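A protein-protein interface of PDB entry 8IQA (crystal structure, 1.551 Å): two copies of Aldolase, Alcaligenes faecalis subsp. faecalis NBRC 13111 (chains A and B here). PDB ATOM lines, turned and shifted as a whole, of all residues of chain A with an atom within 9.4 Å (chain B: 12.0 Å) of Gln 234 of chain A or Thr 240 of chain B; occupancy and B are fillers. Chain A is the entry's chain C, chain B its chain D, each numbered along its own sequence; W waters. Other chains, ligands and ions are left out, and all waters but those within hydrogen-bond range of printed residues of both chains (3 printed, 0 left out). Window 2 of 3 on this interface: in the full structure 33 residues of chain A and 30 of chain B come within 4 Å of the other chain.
NH1 of Arg 21 of chain A lies within hydrogen-bond range of O of Ala 237 of chain B.
NE2 of Gln 234 of chain A sits at hydrogen-bond distance from O of Leu 239 of chain B, 3.2 Å away.
NE2 of Gln 234 of chain A sits at hydrogen-bond distance from O of Thr 240 of chain B, at 2.9 Å.
The backbone carbonyl oxygen (O) of Ala 58 of chain A lies within hydrogen-bond range of the guanidinium group (NE) of Arg 21 of chain A.
O of Ser 230 of chain A is in hydrogen-bond range of OG1 of Thr 233 of chain A, at 2.8 Å.
Among the printed residues, pairs that only touch across the chains: Ala 17 of chain A with Leu 239 of chain B (3.7 Å), Phe 18 of chain A with Leu 239 of chain B (3.7 Å), Arg 21 of chain A with Ile 236 of chain B (3.9 Å), Arg 21 of chain A with Pro 238 of chain B (3.8 Å), Arg 21 of chain A with Leu 239 of chain B (3.6 Å), Ala 58 of chain A with Leu 239 of chain B (3.7 Å), Thr 233 of chain A with Pro 238 of chain B (3.5 Å) and Gln 234 of chain A with Pro 238 of chain B (3.9 Å).
Of the printed residues of chain B, Ala 17 of chain A touches Leu 239.
Of the printed residues of chain B, Arg 21 of chain A touches Ile 236 (3.9 Å), Ala 237 (3.0 Å), Pro 238 (3.8 Å) and Leu 239 (3.6 Å).
Of the printed residues of chain B, Ala 58 of chain A touches Leu 239 (3.7 Å).
No residue of chain B comes within 4 Å of Ser 230 of chain A.
Thr 233 of chain A touches just one residue of chain B: Pro 238 (3.5 Å).
Gln 234 of chain A touches just these residues of chain B: Pro 238 (3.9 Å), Leu 239 (3.2 Å) and Thr 240 (2.9 Å).
Printed residues of chain A within 4 Å of Ile 236 of chain B: Arg 21.
Of the printed residues of chain A, Pro 238 of chain B touches Arg 21, Thr 233 and Gln 234.
The nearest printed residue of chain A that does not touch Ile 236 of chain B is Ala 58 of chain A (5.9 Å).
Of the 5 printed residues of chain B, 5 touch a printed residue of chain A.
Printed residues of chain B that touch a printed residue of chain A: Ile 236, Ala 237, Pro 238, Leu 239 and Thr 240.
Of the 21 printed residues of chain A, 6 touch a printed residue of chain B.
Hydrophobic or aromatic side chains of chain A within 4 Å of the printed part of chain B: Ala 17 and Phe 18.
Along chain A the printed residues that touch a printed residue of chain B span positions 17 to 234.
Among the printed residues, 11 pairs touch across the chains.
Among the printed residues, no Asp or Glu carboxylate lies within 4 Å of a Lys or Arg side-chain nitrogen of the other chain.
2 positions are printed for both chains.
Water W3 bridges O of Ala 237 of chain B and NH2 of Arg 21 of chain A.
Water W1 lies within hydrogen-bond range of N of Leu 239 of chain B and OG1 of Thr 233 of chain A.
Water W2 bridges the backbone carbonyl oxygen (O) of Leu 239 of chain B (2.9 Å) and the backbone carbonyl oxygen (O) of Gln 234 of chain A (3.3 Å).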
ATOM      1  N   GLU A  14       9.733 -10.548   7.824  1.00  0.00           N
ATOM      2  CA  GLU A  14      10.276  -9.981   9.048  1.00  0.00           C
ATOM      3  C   GLU A  14       9.344  -8.934   9.604  1.00  0.00           C
ATOM      4  O   GLU A  14       9.140  -8.885  10.819  1.00  0.00           O
ATOM      5  CB  GLU A  14      11.666  -9.356   8.793  1.00  0.00           C
ATOM      6  N   ALA A  17       6.458 -10.720  11.202  1.00  0.00           N
ATOM      7  CA  ALA A  17       6.844 -11.343  12.491  1.00  0.00           C
ATOM      8  C   ALA A  17       6.829 -10.282  13.601  1.00  0.00           C
ATOM      9  O   ALA A  17       6.242 -10.501  14.667  1.00  0.00           O
ATOM     10  CB  ALA A  17       8.236 -11.964  12.379  1.00  0.00           C
ATOM     11  N   PHE A  18       7.414  -9.084  13.326  1.00  0.00           N
ATOM     12  CA  PHE A  18       7.378  -8.004  14.324  1.00  0.00           C
ATOM     13  C   PHE A  18       5.961  -7.569  14.611  1.00  0.00           C
ATOM     14  O   PHE A  18       5.632  -7.380  15.766  1.00  0.00           O
ATOM     15  CB  PHE A  18       8.259  -6.794  13.918  1.00  0.00           C
ATOM     16  CG  PHE A  18       9.699  -7.024  14.316  1.00  0.00           C
ATOM     17  CD1 PHE A  18      10.085  -6.976  15.652  1.00  0.00           C
ATOM     18  CD2 PHE A  18      10.643  -7.390  13.374  1.00  0.00           C
ATOM     19  CE1 PHE A  18      11.399  -7.243  16.030  1.00  0.00           C
ATOM     20  CE2 PHE A  18      11.959  -7.653  13.754  1.00  0.00           C
ATOM     21  CZ  PHE A  18      12.327  -7.577  15.082  1.00  0.00           C
ATOM     22  N   ARG A  21       4.462 -10.016  17.073  1.00  0.00           N
ATOM     23  CA  ARG A  21       4.998  -9.820  18.434  1.00  0.00           C
ATOM     24  C   ARG A  21       4.432  -8.549  19.084  1.00  0.00           C
ATOM     25  O   ARG A  21       4.233  -8.517  20.307  1.00  0.00           O
ATOM     26  CB  ARG A  21       6.534  -9.777  18.426  1.00  0.00           C
ATOM     27  CG  ARG A  21       7.195 -11.042  17.883  1.00  0.00           C
ATOM     28  CD  ARG A  21       6.656 -12.344  18.482  1.00  0.00           C
ATOM     29  NE  ARG A  21       7.362 -13.499  17.956  1.00  0.00           N
ATOM     30  CZ  ARG A  21       8.373 -14.119  18.570  1.00  0.00           C
ATOM     31  NH1 ARG A  21       8.785 -13.710  19.768  1.00  0.00           N
ATOM     32  NH2 ARG A  21       8.965 -15.155  17.998  1.00  0.00           N
ATOM     33  N   ILE A  22       4.229  -7.480  18.275  1.00  0.00           N
ATOM     34  CA  ILE A  22       3.676  -6.235  18.812  1.00  0.00           C
ATOM     35  C   ILE A  22       2.222  -6.435  19.244  1.00  0.00           C
ATOM     36  O   ILE A  22       1.848  -5.998  20.348  1.00  0.00           O
ATOM     37  CB  ILE A  22       3.790  -5.109  17.782  1.00  0.00           C
ATOM     38  CG1 ILE A  22       5.280  -4.757  17.527  1.00  0.00           C
ATOM     39  CG2 ILE A  22       2.953  -3.874  18.188  1.00  0.00           C
ATOM     40  CD1 ILE A  22       5.447  -3.913  16.227  1.00  0.00           C
ATOM     41  N   MET A  25       2.278  -8.328  22.462  1.00  0.00           N
ATOM     42  CA  MET A  25       2.758  -7.496  23.563  1.00  0.00           C
ATOM     43  C   MET A  25       1.658  -6.542  24.042  1.00  0.00           C
ATOM     44  O   MET A  25       1.508  -6.276  25.261  1.00  0.00           O
ATOM     45  CB  MET A  25       4.004  -6.734  23.093  1.00  0.00           C
ATOM     46  CG  MET A  25       4.531  -5.758  24.123  1.00  0.00           C
ATOM     47  SD  MET A  25       5.952  -4.821  23.499  1.00  0.00           S
ATOM     48  CE  MET A  25       5.127  -3.837  22.213  1.00  0.00           C
ATOM     49  N   ALA A  58       5.269 -16.095  16.450  1.00  0.00           N
ATOM     50  CA  ALA A  58       5.575 -15.952  15.026  1.00  0.00           C
ATOM     51  C   ALA A  58       7.015 -15.582  14.750  1.00  0.00           C
ATOM     52  O   ALA A  58       7.562 -14.682  15.394  1.00  0.00           O
ATOM     53  CB  ALA A  58       4.647 -14.928  14.406  1.00  0.00           C
ATOM     54  N   THR A  59       7.648 -16.287  13.797  1.00  0.00           N
ATOM     55  CA  THR A  59       8.990 -15.924  13.319  1.00  0.00           C
ATOM     56  C   THR A  59       8.877 -15.729  11.782  1.00  0.00           C
ATOM     57  O   THR A  59       7.886 -16.146  11.194  1.00  0.00           O
ATOM     58  CB  THR A  59      10.026 -17.043  13.621  1.00  0.00           C
ATOM     59  OG1 THR A  59       9.706 -18.208  12.870  1.00  0.00           O
ATOM     60  CG2 THR A  59      10.150 -17.367  15.118  1.00  0.00           C
ATOM     61  N   PRO A  60       9.878 -15.133  11.115  1.00  0.00           N
ATOM     62  CA  PRO A  60       9.751 -14.901   9.664  1.00  0.00           C
ATOM     63  C   PRO A  60       9.407 -16.163   8.852  1.00  0.00           C
ATOM     64  O   PRO A  60       8.591 -16.115   7.934  1.00  0.00           O
ATOM     65  CB  PRO A  60      11.114 -14.312   9.283  1.00  0.00           C
ATOM     66  CG  PRO A  60      11.544 -13.563  10.522  1.00  0.00           C
ATOM     67  CD  PRO A  60      11.097 -14.488  11.661  1.00  0.00           C
ATOM     68  N   PHE A 226       5.889   1.996  14.890  1.00  0.00           N
ATOM     69  CA  PHE A 226       6.018   0.544  14.661  1.00  0.00           C
ATOM     70  C   PHE A 226       7.436   0.086  15.019  1.00  0.00           C
ATOM     71  O   PHE A 226       7.592  -0.949  15.643  1.00  0.00           O
ATOM     72  CB  PHE A 226       5.724   0.217  13.184  1.00  0.00           C
ATOM     73  CG  PHE A 226       5.780  -1.274  12.889  1.00  0.00           C
ATOM     74  CD1 PHE A 226       6.967  -1.877  12.504  1.00  0.00           C
ATOM     75  CD2 PHE A 226       4.629  -2.062  12.953  1.00  0.00           C
ATOM     76  CE1 PHE A 226       7.018  -3.229  12.200  1.00  0.00           C
ATOM     77  CE2 PHE A 226       4.687  -3.419  12.670  1.00  0.00           C
ATOM     78  CZ  PHE A 226       5.883  -3.997  12.279  1.00  0.00           C
ATOM     79  N   ASP A 227       8.464   0.864  14.629  1.00  0.00           N
ATOM     80  CA  ASP A 227       9.842   0.484  14.945  1.00  0.00           C
ATOM     81  C   ASP A 227      10.108   0.544  16.445  1.00  0.00           C
ATOM     82  O   ASP A 227      10.805  -0.307  16.979  1.00  0.00           O
ATOM     83  CB  ASP A 227      10.807   1.379  14.181  1.00  0.00           C
ATOM     84  CG  ASP A 227      10.817   1.103  12.670  1.00  0.00           C
ATOM     85  OD1 ASP A 227      10.185   0.086  12.227  1.00  0.00           O
ATOM     86  OD2 ASP A 227      11.422   1.893  11.938  1.00  0.00           O
ATOM     87  N   TYR A 228       9.520   1.529  17.132  1.00  0.00           N
ATOM     88  CA  TYR A 228       9.657   1.635  18.591  1.00  0.00           C
ATOM     89  C   TYR A 228       9.027   0.388  19.253  1.00  0.00           C
ATOM     90  O   TYR A 228       9.667  -0.271  20.081  1.00  0.00           O
ATOM     91  CB  TYR A 228       8.921   2.890  19.068  1.00  0.00           C
ATOM     92  CG  TYR A 228       8.579   2.879  20.537  1.00  0.00           C
ATOM     93  CD1 TYR A 228       9.569   2.717  21.500  1.00  0.00           C
ATOM     94  CD2 TYR A 228       7.280   3.085  20.969  1.00  0.00           C
ATOM     95  CE1 TYR A 228       9.267   2.714  22.849  1.00  0.00           C
ATOM     96  CE2 TYR A 228       6.969   3.117  22.324  1.00  0.00           C
ATOM     97  CZ  TYR A 228       7.971   2.946  23.260  1.00  0.00           C
ATOM     98  OH  TYR A 228       7.688   3.012  24.597  1.00  0.00           O
ATOM     99  N   TRP A 229       7.770   0.038  18.868  1.00  0.00           N
ATOM    100  CA  TRP A 229       7.120  -1.139  19.448  1.00  0.00           C
ATOM    101  C   TRP A 229       7.939  -2.393  19.132  1.00  0.00           C
ATOM    102  O   TRP A 229       8.057  -3.249  19.987  1.00  0.00           O
ATOM    103  CB  TRP A 229       5.706  -1.302  18.889  1.00  0.00           C
ATOM    104  CG  TRP A 229       4.745  -0.229  19.303  1.00  0.00           C
ATOM    105  CD1 TRP A 229       4.633   0.349  20.534  1.00  0.00           C
ATOM    106  CD2 TRP A 229       3.583   0.163  18.564  1.00  0.00           C
ATOM    107  NE1 TRP A 229       3.516   1.166  20.572  1.00  0.00           N
ATOM    108  CE2 TRP A 229       2.840   1.042  19.384  1.00  0.00           C
ATOM    109  CE3 TRP A 229       3.069  -0.191  17.305  1.00  0.00           C
ATOM    110  CZ2 TRP A 229       1.669   1.652  18.941  1.00  0.00           C
ATOM    111  CZ3 TRP A 229       1.908   0.407  16.862  1.00  0.00           C
ATOM    112  CH2 TRP A 229       1.214   1.308  17.684  1.00  0.00           C
ATOM    113  N   SER A 230       8.542  -2.477  17.916  1.00  0.00           N
ATOM    114  CA  SER A 230       9.381  -3.627  17.543  1.00  0.00           C
ATOM    115  C   SER A 230      10.566  -3.759  18.522  1.00  0.00           C
ATOM    116  O   SER A 230      10.830  -4.846  19.026  1.00  0.00           O
ATOM    117  CB  SER A 230       9.907  -3.467  16.121  1.00  0.00           C
ATOM    118  OG  SER A 230       8.854  -3.539  15.168  1.00  0.00           O
ATOM    119  N   ARG A 231      11.234  -2.637  18.845  1.00  0.00           N
ATOM    120  CA  ARG A 231      12.336  -2.666  19.827  1.00  0.00           C
ATOM    121  C   ARG A 231      11.836  -3.114  21.191  1.00  0.00           C
ATOM    122  O   ARG A 231      12.527  -3.864  21.858  1.00  0.00           O
ATOM    123  CB  ARG A 231      13.017  -1.285  19.926  1.00  0.00           C
ATOM    124  CG  ARG A 231      13.686  -0.873  18.618  1.00  0.00           C
ATOM    125  CD  ARG A 231      14.616   0.358  18.775  1.00  0.00           C
ATOM    126  NE  ARG A 231      13.931   1.517  19.363  1.00  0.00           N
ATOM    127  CZ  ARG A 231      13.267   2.439  18.660  1.00  0.00           C
ATOM    128  NH1 ARG A 231      13.183   2.347  17.331  1.00  0.00           N
ATOM    129  NH2 ARG A 231      12.686   3.462  19.278  1.00  0.00           N
ATOM    130  N   GLN A 232      10.628  -2.682  21.616  1.00  0.00           N
ATOM    131  CA  GLN A 232      10.075  -3.091  22.908  1.00  0.00           C
ATOM    132  C   GLN A 232       9.907  -4.601  22.988  1.00  0.00           C
ATOM    133  O   GLN A 232      10.159  -5.191  24.049  1.00  0.00           O
ATOM    134  CB  GLN A 232       8.697  -2.462  23.161  1.00  0.00           C
ATOM    135  CG  GLN A 232       8.694  -0.951  23.355  1.00  0.00           C
ATOM    136  CD  GLN A 232       7.296  -0.555  23.748  1.00  0.00           C
ATOM    137  OE1 GLN A 232       6.351  -0.785  23.005  1.00  0.00           O
ATOM    138  NE2 GLN A 232       7.121   0.036  24.935  1.00  0.00           N
ATOM    139  N   THR A 233       9.419  -5.238  21.897  1.00  0.00           N
ATOM    140  CA  THR A 233       9.206  -6.702  21.954  1.00  0.00           C
ATOM    141  C   THR A 233      10.537  -7.459  22.191  1.00  0.00           C
ATOM    142  O   THR A 233      10.518  -8.567  22.707  1.00  0.00           O
ATOM    143  CB  THR A 233       8.551  -7.227  20.641  1.00  0.00           C
ATOM    144  OG1 THR A 233       9.475  -7.189  19.573  1.00  0.00           O
ATOM    145  CG2 THR A 233       7.265  -6.510  20.282  1.00  0.00           C
ATOM    146  N   GLN A 234      11.663  -6.901  21.725  1.00  0.00           N
ATOM    147  CA  GLN A 234      12.967  -7.552  21.847  1.00  0.00           C
ATOM    148  C   GLN A 234      13.619  -7.471  23.237  1.00  0.00           C
ATOM    149  O   GLN A 234      14.640  -8.117  23.465  1.00  0.00           O
ATOM    150  CB  GLN A 234      13.911  -7.006  20.801  1.00  0.00           C
ATOM    151  CG  GLN A 234      13.382  -7.247  19.400  1.00  0.00           C
ATOM    152  CD  GLN A 234      14.248  -6.626  18.364  1.00  0.00           C
ATOM    153  OE1 GLN A 234      14.434  -5.408  18.313  1.00  0.00           O
ATOM    154  NE2 GLN A 234      14.774  -7.455  17.496  1.00  0.00           N
ATOM    155  N   GLY A 235      13.028  -6.704  24.145  1.00  0.00           N
ATOM    156  CA  GLY A 235      13.531  -6.565  25.497  1.00  0.00           C
ATOM    157  C   GLY A 235      14.464  -5.382  25.597  1.00  0.00           C
ATOM    158  O   GLY A 235      15.287  -5.157  24.707  1.00  0.00           O
ATOM    159  N   ILE A 236      14.278  -4.569  26.635  1.00  0.00           N
ATOM    160  CA  ILE A 236      15.163  -3.425  26.827  1.00  0.00           C
ATOM    161  C   ILE A 236      15.870  -3.667  28.161  1.00  0.00           C
ATOM    162  O   ILE A 236      15.199  -3.959  29.160  1.00  0.00           O
ATOM    163  CB  ILE A 236      14.379  -2.111  26.821  1.00  0.00           C
ATOM    164  CG1 ILE A 236      13.675  -1.901  25.468  1.00  0.00           C
ATOM    165  CG2 ILE A 236      15.295  -0.946  27.190  1.00  0.00           C
ATOM    166  CD1 ILE A 236      12.474  -0.951  25.570  1.00  0.00           C
ATOM    167  N   ALA A 237      17.186  -3.549  28.181  1.00  0.00           N
ATOM    168  CA  ALA A 237      17.929  -3.755  29.421  1.00  0.00           C
ATOM    169  C   ALA A 237      17.593  -2.642  30.438  1.00  0.00           C
ATOM    170  O   ALA A 237      17.454  -1.460  30.073  1.00  0.00           O
ATOM    171  CB  ALA A 237      19.424  -3.774  29.139  1.00  0.00           C
ATOM    172  N   ILE B 236       8.646 -18.095  25.213  1.00  0.00           N
ATOM    173  CA  ILE B 236       8.949 -17.862  23.801  1.00  0.00           C
ATOM    174  C   ILE B 236      10.052 -16.824  23.748  1.00  0.00           C
ATOM    175  O   ILE B 236       9.929 -15.776  24.373  1.00  0.00           O
ATOM    176  CB  ILE B 236       7.691 -17.387  23.037  1.00  0.00           C
ATOM    177  CG1 ILE B 236       6.567 -18.487  23.106  1.00  0.00           C
ATOM    178  CG2 ILE B 236       8.065 -17.082  21.579  1.00  0.00           C
ATOM    179  CD1 ILE B 236       5.172 -17.922  22.928  1.00  0.00           C
ATOM    180  N   ALA B 237      11.123 -17.102  23.011  1.00  0.00           N
ATOM    181  CA  ALA B 237      12.223 -16.147  22.888  1.00  0.00           C
ATOM    182  C   ALA B 237      11.795 -14.957  22.049  1.00  0.00           C
ATOM    183  O   ALA B 237      11.084 -15.137  21.053  1.00  0.00           O
ATOM    184  CB  ALA B 237      13.418 -16.820  22.221  1.00  0.00           C
ATOM    185  N   PRO B 238      12.242 -13.737  22.399  1.00  0.00           N
ATOM    186  CA  PRO B 238      11.937 -12.589  21.534  1.00  0.00           C
ATOM    187  C   PRO B 238      12.623 -12.717  20.171  1.00  0.00           C
ATOM    188  O   PRO B 238      13.580 -13.475  20.019  1.00  0.00           O
ATOM    189  CB  PRO B 238      12.514 -11.381  22.320  1.00  0.00           C
ATOM    190  CG  PRO B 238      13.578 -11.967  23.194  1.00  0.00           C
ATOM    191  CD  PRO B 238      13.093 -13.363  23.548  1.00  0.00           C
ATOM    192  N   LEU B 239      12.164 -11.940  19.172  1.00  0.00           N
ATOM    193  CA  LEU B 239      12.801 -11.914  17.862  1.00  0.00           C
ATOM    194  C   LEU B 239      14.172 -11.251  18.030  1.00  0.00           C
ATOM    195  O   LEU B 239      14.306 -10.327  18.838  1.00  0.00           O
ATOM    196  CB  LEU B 239      11.963 -11.053  16.876  1.00  0.00           C
ATOM    197  CG  LEU B 239      10.604 -11.608  16.483  1.00  0.00           C
ATOM    198  CD1 LEU B 239       9.886 -10.658  15.582  1.00  0.00           C
ATOM    199  CD2 LEU B 239      10.765 -12.899  15.732  1.00  0.00           C
ATOM    200  N   THR B 240      15.183 -11.721  17.305  1.00  0.00           N
ATOM    201  CA  THR B 240      16.526 -11.145  17.427  1.00  0.00           C
ATOM    202  C   THR B 240      16.654  -9.799  16.723  1.00  0.00           C
ATOM    203  O   THR B 240      15.901  -9.509  15.783  1.00  0.00           O
ATOM    204  CB  THR B 240      17.606 -12.141  16.965  1.00  0.00           C
HETATM  205  O   HOH W   1      10.093 -10.036  19.665  1.00  0.00           O
HETATM  206  O   HOH W   2      16.029  -9.887  21.103  1.00  0.00           O
HETATM  207  O   HOH W   3      11.215 -16.668  18.818  1.00  0.00           O
